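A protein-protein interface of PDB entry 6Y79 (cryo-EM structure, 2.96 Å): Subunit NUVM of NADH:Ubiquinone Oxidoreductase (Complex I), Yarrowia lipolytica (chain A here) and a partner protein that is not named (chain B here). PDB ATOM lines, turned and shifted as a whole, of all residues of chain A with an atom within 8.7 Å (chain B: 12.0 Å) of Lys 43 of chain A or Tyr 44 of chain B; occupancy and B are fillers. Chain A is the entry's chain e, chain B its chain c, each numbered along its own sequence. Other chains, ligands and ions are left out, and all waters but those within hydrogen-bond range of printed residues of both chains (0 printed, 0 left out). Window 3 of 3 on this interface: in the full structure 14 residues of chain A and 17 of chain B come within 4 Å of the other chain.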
ATOM      1  N   PHE A  36     -28.273  23.877 -18.755  1.00  0.00           N
ATOM      2  CA  PHE A  36     -27.737  22.990 -19.778  1.00  0.00           C
ATOM      3  C   PHE A  36     -27.402  21.622 -19.204  1.00  0.00           C
ATOM      4  O   PHE A  36     -27.710  20.590 -19.816  1.00  0.00           O
ATOM      5  CB  PHE A  36     -26.506  23.633 -20.401  1.00  0.00           C
ATOM      6  CG  PHE A  36     -25.876  22.809 -21.468  1.00  0.00           C
ATOM      7  CD1 PHE A  36     -26.471  22.698 -22.708  1.00  0.00           C
ATOM      8  CD2 PHE A  36     -24.690  22.140 -21.234  1.00  0.00           C
ATOM      9  CE1 PHE A  36     -25.892  21.934 -23.697  1.00  0.00           C
ATOM     10  CE2 PHE A  36     -24.109  21.373 -22.217  1.00  0.00           C
ATOM     11  CZ  PHE A  36     -24.712  21.270 -23.451  1.00  0.00           C
ATOM     12  N   TRP A  37     -26.766  21.590 -18.027  1.00  0.00           N
ATOM     13  CA  TRP A  37     -26.411  20.323 -17.407  1.00  0.00           C
ATOM     14  C   TRP A  37     -27.642  19.549 -16.973  1.00  0.00           C
ATOM     15  O   TRP A  37     -27.684  18.321 -17.124  1.00  0.00           O
ATOM     16  CB  TRP A  37     -25.499  20.565 -16.212  1.00  0.00           C
ATOM     17  CG  TRP A  37     -25.042  19.305 -15.580  1.00  0.00           C
ATOM     18  CD1 TRP A  37     -25.446  18.795 -14.386  1.00  0.00           C
ATOM     19  CD2 TRP A  37     -24.106  18.375 -16.120  1.00  0.00           C
ATOM     20  NE1 TRP A  37     -24.807  17.606 -14.142  1.00  0.00           N
ATOM     21  CE2 TRP A  37     -23.979  17.327 -15.195  1.00  0.00           C
ATOM     22  CE3 TRP A  37     -23.353  18.331 -17.296  1.00  0.00           C
ATOM     23  CZ2 TRP A  37     -23.133  16.247 -15.408  1.00  0.00           C
ATOM     24  CZ3 TRP A  37     -22.514  17.260 -17.505  1.00  0.00           C
ATOM     25  CH2 TRP A  37     -22.411  16.232 -16.568  1.00  0.00           C
ATOM     26  N   MET A  38     -28.663  20.248 -16.468  1.00  0.00           N
ATOM     27  CA  MET A  38     -29.893  19.567 -16.096  1.00  0.00           C
ATOM     28  C   MET A  38     -30.621  19.036 -17.320  1.00  0.00           C
ATOM     29  O   MET A  38     -31.164  17.934 -17.270  1.00  0.00           O
ATOM     30  CB  MET A  38     -30.791  20.490 -15.275  1.00  0.00           C
ATOM     31  CG  MET A  38     -30.283  20.707 -13.860  1.00  0.00           C
ATOM     32  SD  MET A  38     -31.212  21.958 -12.967  1.00  0.00           S
ATOM     33  CE  MET A  38     -32.643  21.010 -12.484  1.00  0.00           C
ATOM     34  N   PHE A  39     -30.593  19.765 -18.440  1.00  0.00           N
ATOM     35  CA  PHE A  39     -31.220  19.250 -19.656  1.00  0.00           C
ATOM     36  C   PHE A  39     -30.490  18.026 -20.190  1.00  0.00           C
ATOM     37  O   PHE A  39     -31.134  17.064 -20.618  1.00  0.00           O
ATOM     38  CB  PHE A  39     -31.279  20.332 -20.729  1.00  0.00           C
ATOM     39  CG  PHE A  39     -32.307  21.385 -20.469  1.00  0.00           C
ATOM     40  CD1 PHE A  39     -33.321  21.182 -19.544  1.00  0.00           C
ATOM     41  CD2 PHE A  39     -32.259  22.587 -21.150  1.00  0.00           C
ATOM     42  CE1 PHE A  39     -34.260  22.157 -19.306  1.00  0.00           C
ATOM     43  CE2 PHE A  39     -33.197  23.566 -20.917  1.00  0.00           C
ATOM     44  CZ  PHE A  39     -34.199  23.349 -19.993  1.00  0.00           C
ATOM     45  N   LEU A  40     -29.157  18.025 -20.135  1.00  0.00           N
ATOM     46  CA  LEU A  40     -28.399  16.875 -20.620  1.00  0.00           C
ATOM     47  C   LEU A  40     -28.618  15.656 -19.732  1.00  0.00           C
ATOM     48  O   LEU A  40     -28.685  14.520 -20.220  1.00  0.00           O
ATOM     49  CB  LEU A  40     -26.914  17.226 -20.703  1.00  0.00           C
ATOM     50  CG  LEU A  40     -25.996  16.300 -21.494  1.00  0.00           C
ATOM     51  CD1 LEU A  40     -25.052  17.122 -22.320  1.00  0.00           C
ATOM     52  CD2 LEU A  40     -25.202  15.440 -20.558  1.00  0.00           C
ATOM     53  N   ARG A  41     -28.755  15.870 -18.426  1.00  0.00           N
ATOM     54  CA  ARG A  41     -28.952  14.736 -17.536  1.00  0.00           C
ATOM     55  C   ARG A  41     -30.399  14.257 -17.481  1.00  0.00           C
ATOM     56  O   ARG A  41     -30.622  13.103 -17.111  1.00  0.00           O
ATOM     57  CB  ARG A  41     -28.445  15.077 -16.138  1.00  0.00           C
ATOM     58  CG  ARG A  41     -26.934  15.253 -16.053  1.00  0.00           C
ATOM     59  CD  ARG A  41     -26.200  13.924 -16.157  1.00  0.00           C
ATOM     60  NE  ARG A  41     -25.598  13.708 -17.470  1.00  0.00           N
ATOM     61  CZ  ARG A  41     -25.256  12.514 -17.944  1.00  0.00           C
ATOM     62  NH1 ARG A  41     -24.714  12.400 -19.147  1.00  0.00           N
ATOM     63  NH2 ARG A  41     -25.467  11.428 -17.216  1.00  0.00           N
ATOM     64  N   ILE A  42     -31.385  15.096 -17.830  1.00  0.00           N
ATOM     65  CA  ILE A  42     -32.718  14.567 -18.131  1.00  0.00           C
ATOM     66  C   ILE A  42     -32.675  13.778 -19.430  1.00  0.00           C
ATOM     67  O   ILE A  42     -33.278  12.699 -19.539  1.00  0.00           O
ATOM     68  CB  ILE A  42     -33.788  15.678 -18.231  1.00  0.00           C
ATOM     69  CG1 ILE A  42     -33.936  16.494 -16.953  1.00  0.00           C
ATOM     70  CG2 ILE A  42     -35.163  15.082 -18.522  1.00  0.00           C
ATOM     71  CD1 ILE A  42     -34.304  15.718 -15.788  1.00  0.00           C
ATOM     72  N   LYS A  43     -31.954  14.311 -20.429  1.00  0.00           N
ATOM     73  CA  LYS A  43     -31.900  13.715 -21.754  1.00  0.00           C
ATOM     74  C   LYS A  43     -31.318  12.305 -21.714  1.00  0.00           C
ATOM     75  O   LYS A  43     -31.918  11.369 -22.243  1.00  0.00           O
ATOM     76  CB  LYS A  43     -31.074  14.611 -22.673  1.00  0.00           C
ATOM     77  CG  LYS A  43     -30.794  14.013 -24.031  1.00  0.00           C
ATOM     78  CD  LYS A  43     -29.339  14.277 -24.411  1.00  0.00           C
ATOM     79  CE  LYS A  43     -28.933  13.527 -25.664  1.00  0.00           C
ATOM     80  NZ  LYS A  43     -29.074  14.386 -26.873  1.00  0.00           N
ATOM     81  N   GLU A  44     -30.180  12.112 -21.059  1.00  0.00           N
ATOM     82  CA  GLU A  44     -29.552  10.795 -21.102  1.00  0.00           C
ATOM     83  C   GLU A  44     -30.152   9.825 -20.083  1.00  0.00           C
ATOM     84  O   GLU A  44     -30.182   8.626 -20.341  1.00  0.00           O
ATOM     85  CB  GLU A  44     -28.035  10.984 -20.932  1.00  0.00           C
ATOM     86  CG  GLU A  44     -27.117   9.775 -20.782  1.00  0.00           C
ATOM     87  CD  GLU A  44     -27.407   8.575 -21.663  1.00  0.00           C
ATOM     88  OE1 GLU A  44     -27.321   7.461 -21.110  1.00  0.00           O
ATOM     89  OE2 GLU A  44     -27.657   8.711 -22.881  1.00  0.00           O
ATOM     90  N   GLU A  45     -30.706  10.299 -18.974  1.00  0.00           N
ATOM     91  CA  GLU A  45     -31.159   9.392 -17.924  1.00  0.00           C
ATOM     92  C   GLU A  45     -32.674   9.171 -17.979  1.00  0.00           C
ATOM     93  O   GLU A  45     -33.216   8.513 -17.097  1.00  0.00           O
ATOM     94  CB  GLU A  45     -30.713   9.901 -16.547  1.00  0.00           C
ATOM     95  CG  GLU A  45     -30.514   8.814 -15.499  1.00  0.00           C
ATOM     96  CD  GLU A  45     -30.330   9.361 -14.092  1.00  0.00           C
ATOM     97  OE1 GLU A  45     -30.052  10.574 -13.948  1.00  0.00           O
ATOM     98  OE2 GLU A  45     -30.569   8.590 -13.139  1.00  0.00           O
ATOM     99  N   TYR A  46     -33.337   9.629 -19.068  1.00  0.00           N
ATOM    100  CA  TYR A  46     -34.804   9.680 -19.180  1.00  0.00           C
ATOM    101  C   TYR A  46     -35.550   8.391 -18.797  1.00  0.00           C
ATOM    102  O   TYR A  46     -36.419   8.466 -17.902  1.00  0.00           O
ATOM    103  CB  TYR A  46     -35.179  10.161 -20.598  1.00  0.00           C
ATOM    104  CG  TYR A  46     -36.659  10.334 -20.861  1.00  0.00           C
ATOM    105  CD1 TYR A  46     -37.310  11.511 -20.510  1.00  0.00           C
ATOM    106  CD2 TYR A  46     -37.402   9.327 -21.477  1.00  0.00           C
ATOM    107  CE1 TYR A  46     -38.659  11.683 -20.755  1.00  0.00           C
ATOM    108  CE2 TYR A  46     -38.759   9.487 -21.717  1.00  0.00           C
ATOM    109  CZ  TYR A  46     -39.378  10.665 -21.350  1.00  0.00           C
ATOM    110  OH  TYR A  46     -40.720  10.833 -21.593  1.00  0.00           O
ATOM    111  N   PRO A  47     -35.240   7.191 -19.343  1.00  0.00           N
ATOM    112  CA  PRO A  47     -36.016   6.012 -18.917  1.00  0.00           C
ATOM    113  C   PRO A  47     -35.684   5.540 -17.512  1.00  0.00           C
ATOM    114  O   PRO A  47     -36.523   4.893 -16.876  1.00  0.00           O
ATOM    115  CB  PRO A  47     -35.651   4.956 -19.966  1.00  0.00           C
ATOM    116  CG  PRO A  47     -34.262   5.271 -20.302  1.00  0.00           C
ATOM    117  CD  PRO A  47     -34.195   6.773 -20.314  1.00  0.00           C
ATOM    118  N   ALA A  48     -34.488   5.840 -17.005  1.00  0.00           N
ATOM    119  CA  ALA A  48     -34.176   5.535 -15.614  1.00  0.00           C
ATOM    120  C   ALA A  48     -34.739   6.603 -14.687  1.00  0.00           C
ATOM    121  O   ALA A  48     -35.248   6.288 -13.607  1.00  0.00           O
ATOM    122  CB  ALA A  48     -32.665   5.403 -15.432  1.00  0.00           C
ATOM    123  N   MET A  49     -34.644   7.873 -15.105  1.00  0.00           N
ATOM    124  CA  MET A  49     -35.110   9.023 -14.326  1.00  0.00           C
ATOM    125  C   MET A  49     -36.586   8.936 -14.003  1.00  0.00           C
ATOM    126  O   MET A  49     -36.982   9.000 -12.832  1.00  0.00           O
ATOM    127  CB  MET A  49     -34.870  10.314 -15.105  1.00  0.00           C
ATOM    128  CG  MET A  49     -35.094  11.576 -14.338  1.00  0.00           C
ATOM    129  SD  MET A  49     -33.621  11.855 -13.372  1.00  0.00           S
ATOM    130  CE  MET A  49     -32.555  12.713 -14.534  1.00  0.00           C
ATOM    131  N   GLY B  35     -32.083  30.959 -21.549  1.00  0.00           N
ATOM    132  CA  GLY B  35     -32.096  31.269 -22.968  1.00  0.00           C
ATOM    133  C   GLY B  35     -30.831  30.878 -23.704  1.00  0.00           C
ATOM    134  O   GLY B  35     -30.865  30.636 -24.913  1.00  0.00           O
ATOM    135  N   ILE B  36     -29.697  30.837 -23.010  1.00  0.00           N
ATOM    136  CA  ILE B  36     -28.491  30.349 -23.667  1.00  0.00           C
ATOM    137  C   ILE B  36     -28.443  28.830 -23.617  1.00  0.00           C
ATOM    138  O   ILE B  36     -27.967  28.177 -24.553  1.00  0.00           O
ATOM    139  CB  ILE B  36     -27.244  30.993 -23.035  1.00  0.00           C
ATOM    140  CG1 ILE B  36     -27.405  32.511 -22.996  1.00  0.00           C
ATOM    141  CG2 ILE B  36     -25.989  30.627 -23.814  1.00  0.00           C
ATOM    142  CD1 ILE B  36     -26.275  33.232 -22.294  1.00  0.00           C
ATOM    143  N   ALA B  37     -28.974  28.242 -22.544  1.00  0.00           N
ATOM    144  CA  ALA B  37     -28.911  26.797 -22.397  1.00  0.00           C
ATOM    145  C   ALA B  37     -29.874  26.087 -23.330  1.00  0.00           C
ATOM    146  O   ALA B  37     -29.610  24.945 -23.708  1.00  0.00           O
ATOM    147  CB  ALA B  37     -29.190  26.385 -20.959  1.00  0.00           C
ATOM    148  N   VAL B  38     -30.973  26.734 -23.732  1.00  0.00           N
ATOM    149  CA  VAL B  38     -31.868  26.061 -24.671  1.00  0.00           C
ATOM    150  C   VAL B  38     -31.221  25.945 -26.047  1.00  0.00           C
ATOM    151  O   VAL B  38     -31.327  24.903 -26.702  1.00  0.00           O
ATOM    152  CB  VAL B  38     -33.249  26.748 -24.738  1.00  0.00           C
ATOM    153  CG1 VAL B  38     -34.032  26.485 -23.461  1.00  0.00           C
ATOM    154  CG2 VAL B  38     -33.138  28.242 -25.001  1.00  0.00           C
ATOM    155  N   VAL B  39     -30.465  26.958 -26.471  1.00  0.00           N
ATOM    156  CA  VAL B  39     -29.830  26.893 -27.782  1.00  0.00           C
ATOM    157  C   VAL B  39     -28.551  26.058 -27.717  1.00  0.00           C
ATOM    158  O   VAL B  39     -28.209  25.358 -28.676  1.00  0.00           O
ATOM    159  CB  VAL B  39     -29.597  28.321 -28.316  1.00  0.00           C
ATOM    160  CG1 VAL B  39     -28.901  28.325 -29.668  1.00  0.00           C
ATOM    161  CG2 VAL B  39     -30.930  29.030 -28.441  1.00  0.00           C
ATOM    162  N   ALA B  40     -27.856  26.061 -26.569  1.00  0.00           N
ATOM    163  CA  ALA B  40     -26.720  25.155 -26.398  1.00  0.00           C
ATOM    164  C   ALA B  40     -27.167  23.699 -26.359  1.00  0.00           C
ATOM    165  O   ALA B  40     -26.490  22.824 -26.914  1.00  0.00           O
ATOM    166  CB  ALA B  40     -25.951  25.503 -25.130  1.00  0.00           C
ATOM    167  N   PHE B  41     -28.323  23.429 -25.751  1.00  0.00           N
ATOM    168  CA  PHE B  41     -28.895  22.093 -25.782  1.00  0.00           C
ATOM    169  C   PHE B  41     -29.371  21.720 -27.178  1.00  0.00           C
ATOM    170  O   PHE B  41     -29.221  20.565 -27.579  1.00  0.00           O
ATOM    171  CB  PHE B  41     -30.043  22.003 -24.780  1.00  0.00           C
ATOM    172  CG  PHE B  41     -30.640  20.642 -24.671  1.00  0.00           C
ATOM    173  CD1 PHE B  41     -29.894  19.586 -24.177  1.00  0.00           C
ATOM    174  CD2 PHE B  41     -31.952  20.417 -25.049  1.00  0.00           C
ATOM    175  CE1 PHE B  41     -30.442  18.325 -24.070  1.00  0.00           C
ATOM    176  CE2 PHE B  41     -32.508  19.159 -24.943  1.00  0.00           C
ATOM    177  CZ  PHE B  41     -31.751  18.112 -24.453  1.00  0.00           C
ATOM    178  N   GLY B  42     -29.928  22.672 -27.931  1.00  0.00           N
ATOM    179  CA  GLY B  42     -30.285  22.392 -29.314  1.00  0.00           C
ATOM    180  C   GLY B  42     -29.073  22.123 -30.188  1.00  0.00           C
ATOM    181  O   GLY B  42     -29.117  21.276 -31.086  1.00  0.00           O
ATOM    182  N   ALA B  43     -27.971  22.824 -29.921  1.00  0.00           N
ATOM    183  CA  ALA B  43     -26.716  22.556 -30.607  1.00  0.00           C
ATOM    184  C   ALA B  43     -26.183  21.174 -30.262  1.00  0.00           C
ATOM    185  O   ALA B  43     -25.670  20.471 -31.136  1.00  0.00           O
ATOM    186  CB  ALA B  43     -25.685  23.627 -30.257  1.00  0.00           C
ATOM    187  N   TYR B  44     -26.310  20.761 -28.996  1.00  0.00           N
ATOM    188  CA  TYR B  44     -25.866  19.422 -28.611  1.00  0.00           C
ATOM    189  C   TYR B  44     -26.760  18.339 -29.213  1.00  0.00           C
ATOM    190  O   TYR B  44     -26.270  17.265 -29.583  1.00  0.00           O
ATOM    191  CB  TYR B  44     -25.821  19.297 -27.089  1.00  0.00           C
ATOM    192  CG  TYR B  44     -25.342  17.948 -26.600  1.00  0.00           C
ATOM    193  CD1 TYR B  44     -23.996  17.611 -26.647  1.00  0.00           C
ATOM    194  CD2 TYR B  44     -26.236  17.014 -26.091  1.00  0.00           C
ATOM    195  CE1 TYR B  44     -23.554  16.378 -26.202  1.00  0.00           C
ATOM    196  CE2 TYR B  44     -25.805  15.779 -25.645  1.00  0.00           C
ATOM    197  CZ  TYR B  44     -24.463  15.467 -25.701  1.00  0.00           C
ATOM    198  OH  TYR B  44     -24.030  14.239 -25.256  1.00  0.00           O
ATOM    199  N   LEU B  45     -28.067  18.604 -29.315  1.00  0.00           N
ATOM    200  CA  LEU B  45     -28.986  17.672 -29.968  1.00  0.00           C
ATOM    201  C   LEU B  45     -28.659  17.529 -31.450  1.00  0.00           C
ATOM    202  O   LEU B  45     -28.666  16.419 -31.995  1.00  0.00           O
ATOM    203  CB  LEU B  45     -30.436  18.136 -29.802  1.00  0.00           C
ATOM    204  CG  LEU B  45     -31.187  18.136 -28.468  1.00  0.00           C
ATOM    205  CD1 LEU B  45     -32.545  18.819 -28.636  1.00  0.00           C
ATOM    206  CD2 LEU B  45     -31.350  16.736 -27.883  1.00  0.00           C
ATOM    207  N   ALA B  46     -28.369  18.650 -32.117  1.00  0.00           N
ATOM    208  CA  ALA B  46     -28.035  18.608 -33.534  1.00  0.00           C
ATOM    209  C   ALA B  46     -26.644  18.043 -33.785  1.00  0.00           C
ATOM    210  O   ALA B  46     -26.401  17.489 -34.862  1.00  0.00           O
ATOM    211  CB  ALA B  46     -28.145  20.006 -34.137  1.00  0.00           C
ATOM    212  N   ALA B  47     -25.733  18.164 -32.822  1.00  0.00           N
ATOM    213  CA  ALA B  47     -24.373  17.678 -32.990  1.00  0.00           C
ATOM    214  C   ALA B  47     -24.176  16.258 -32.487  1.00  0.00           C
ATOM    215  O   ALA B  47     -23.101  15.686 -32.704  1.00  0.00           O
ATOM    216  CB  ALA B  47     -23.389  18.607 -32.272  1.00  0.00           C
ATOM    217  N   GLU B  48     -25.172  15.695 -31.793  1.00  0.00           N
ATOM    218  CA  GLU B  48     -25.132  14.282 -31.428  1.00  0.00           C
ATOM    219  C   GLU B  48     -25.116  13.393 -32.665  1.00  0.00           C
ATOM    220  O   GLU B  48     -24.373  12.406 -32.715  1.00  0.00           O
ATOM    221  CB  GLU B  48     -26.333  13.941 -30.543  1.00  0.00           C
ATOM    222  CG  GLU B  48     -26.199  12.659 -29.726  1.00  0.00           C
ATOM    223  CD  GLU B  48     -26.619  11.412 -30.494  1.00  0.00           C
ATOM    224  OE1 GLU B  48     -27.554  11.504 -31.318  1.00  0.00           O
ATOM    225  OE2 GLU B  48     -26.009  10.345 -30.273  1.00  0.00           O
ATOM    226  N   LYS B  49     -25.926  13.735 -33.662  1.00  0.00           N
ATOM    227  CA  LYS B  49     -26.103  12.948 -34.878  1.00  0.00           C
ATOM    228  C   LYS B  49     -24.835  12.838 -35.724  1.00  0.00           C
ATOM    229  O   LYS B  49     -24.756  12.023 -36.643  1.00  0.00           O
ATOM    230  CB  LYS B  49     -27.220  13.565 -35.717  1.00  0.00           C
ATOM    231  CG  LYS B  49     -28.569  13.567 -35.032  1.00  0.00           C
ATOM    232  CD  LYS B  49     -29.658  14.099 -35.954  1.00  0.00           C
ATOM    233  CE  LYS B  49     -29.583  15.610 -36.097  1.00  0.00           C
ATOM    234  NZ  LYS B  49     -30.716  16.138 -36.904  1.00  0.00           N
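Of the printed residues of chain B, Lys 43 of chain A touches Phe 41, Tyr 44 and Leu 45.
Of the printed residues of chain A, Tyr 44 of chain B touches Leu 40 and Lys 43.
Of chain B, only Tyr 44 (3.7 Å) comes within 4 Å of Leu 40 of chain A.
No residue of chain B comes within 4 Å of Arg 41 of chain A.
No residue of chain B comes within 4 Å of Ile 42 of chain A.
No residue of chain B comes within 4 Å of Glu 44 of chain A.
Of the printed residues of chain A, Phe 41 of chain B touches Phe 36 (3.5 Å), Phe 39 (3.7 Å) and Lys 43 (3.99 Å).
Of the printed residues of chain A, Val 38 of chain B touches Phe 39 (3.96 Å).
Of the printed residues of chain A, Ala 37 of chain B touches Phe 36.
The nearest printed residue of chain B that does not touch Lys 43 of chain A is Glu 48 of chain B (4.4 Å).
The nearest residue of chain A that does not touch Tyr 44 of chain B is Phe 36 of chain A (4.3 Å).
The nearest printed residue of chain B that does not touch Phe 39 of chain A is Ala 37 of chain B (4.4 Å).
Hydrophobic or aromatic side chains of chain A within 4 Å of the printed part of chain B: Phe 36, Phe 39 and Leu 40.
Of the 15 printed residues of chain B, 6 touch a printed residue of chain A.
Hydrophobic or aromatic side chains of chain B within 4 Å of the printed part of chain A: Ala 37, Val 38, Ala 40, Phe 41, Tyr 44 and Leu 45.
Among the printed residues, 9 pairs touch across the chains.
Ala 37 of chain B touches Phe 36 of chain A (CB to N, 3.5 Å).
O of Ala 40 of chain B touches CE1 of Phe 36 of chain A (3.4 Å).
Phe 36 of chain A touches Phe 41 of chain B (CE1 to N, 3.5 Å).
CE2 of Phe 39 of chain A touches CG1 of Val 38 of chain B, at 3.96 Å.
O of Phe 39 of chain A touches CE1 of Phe 41 of chain B, at 3.7 Å.
CD1 of Leu 40 of chain A touches CE2 of Tyr 44 of chain B (3.7 Å).
Phe 41 of chain B touches Lys 43 of chain A (CZ to CB, 3.99 Å).
Tyr 44 of chain B touches Lys 43 of chain A.
Leu 45 of chain B touches Lys 43 of chain A.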
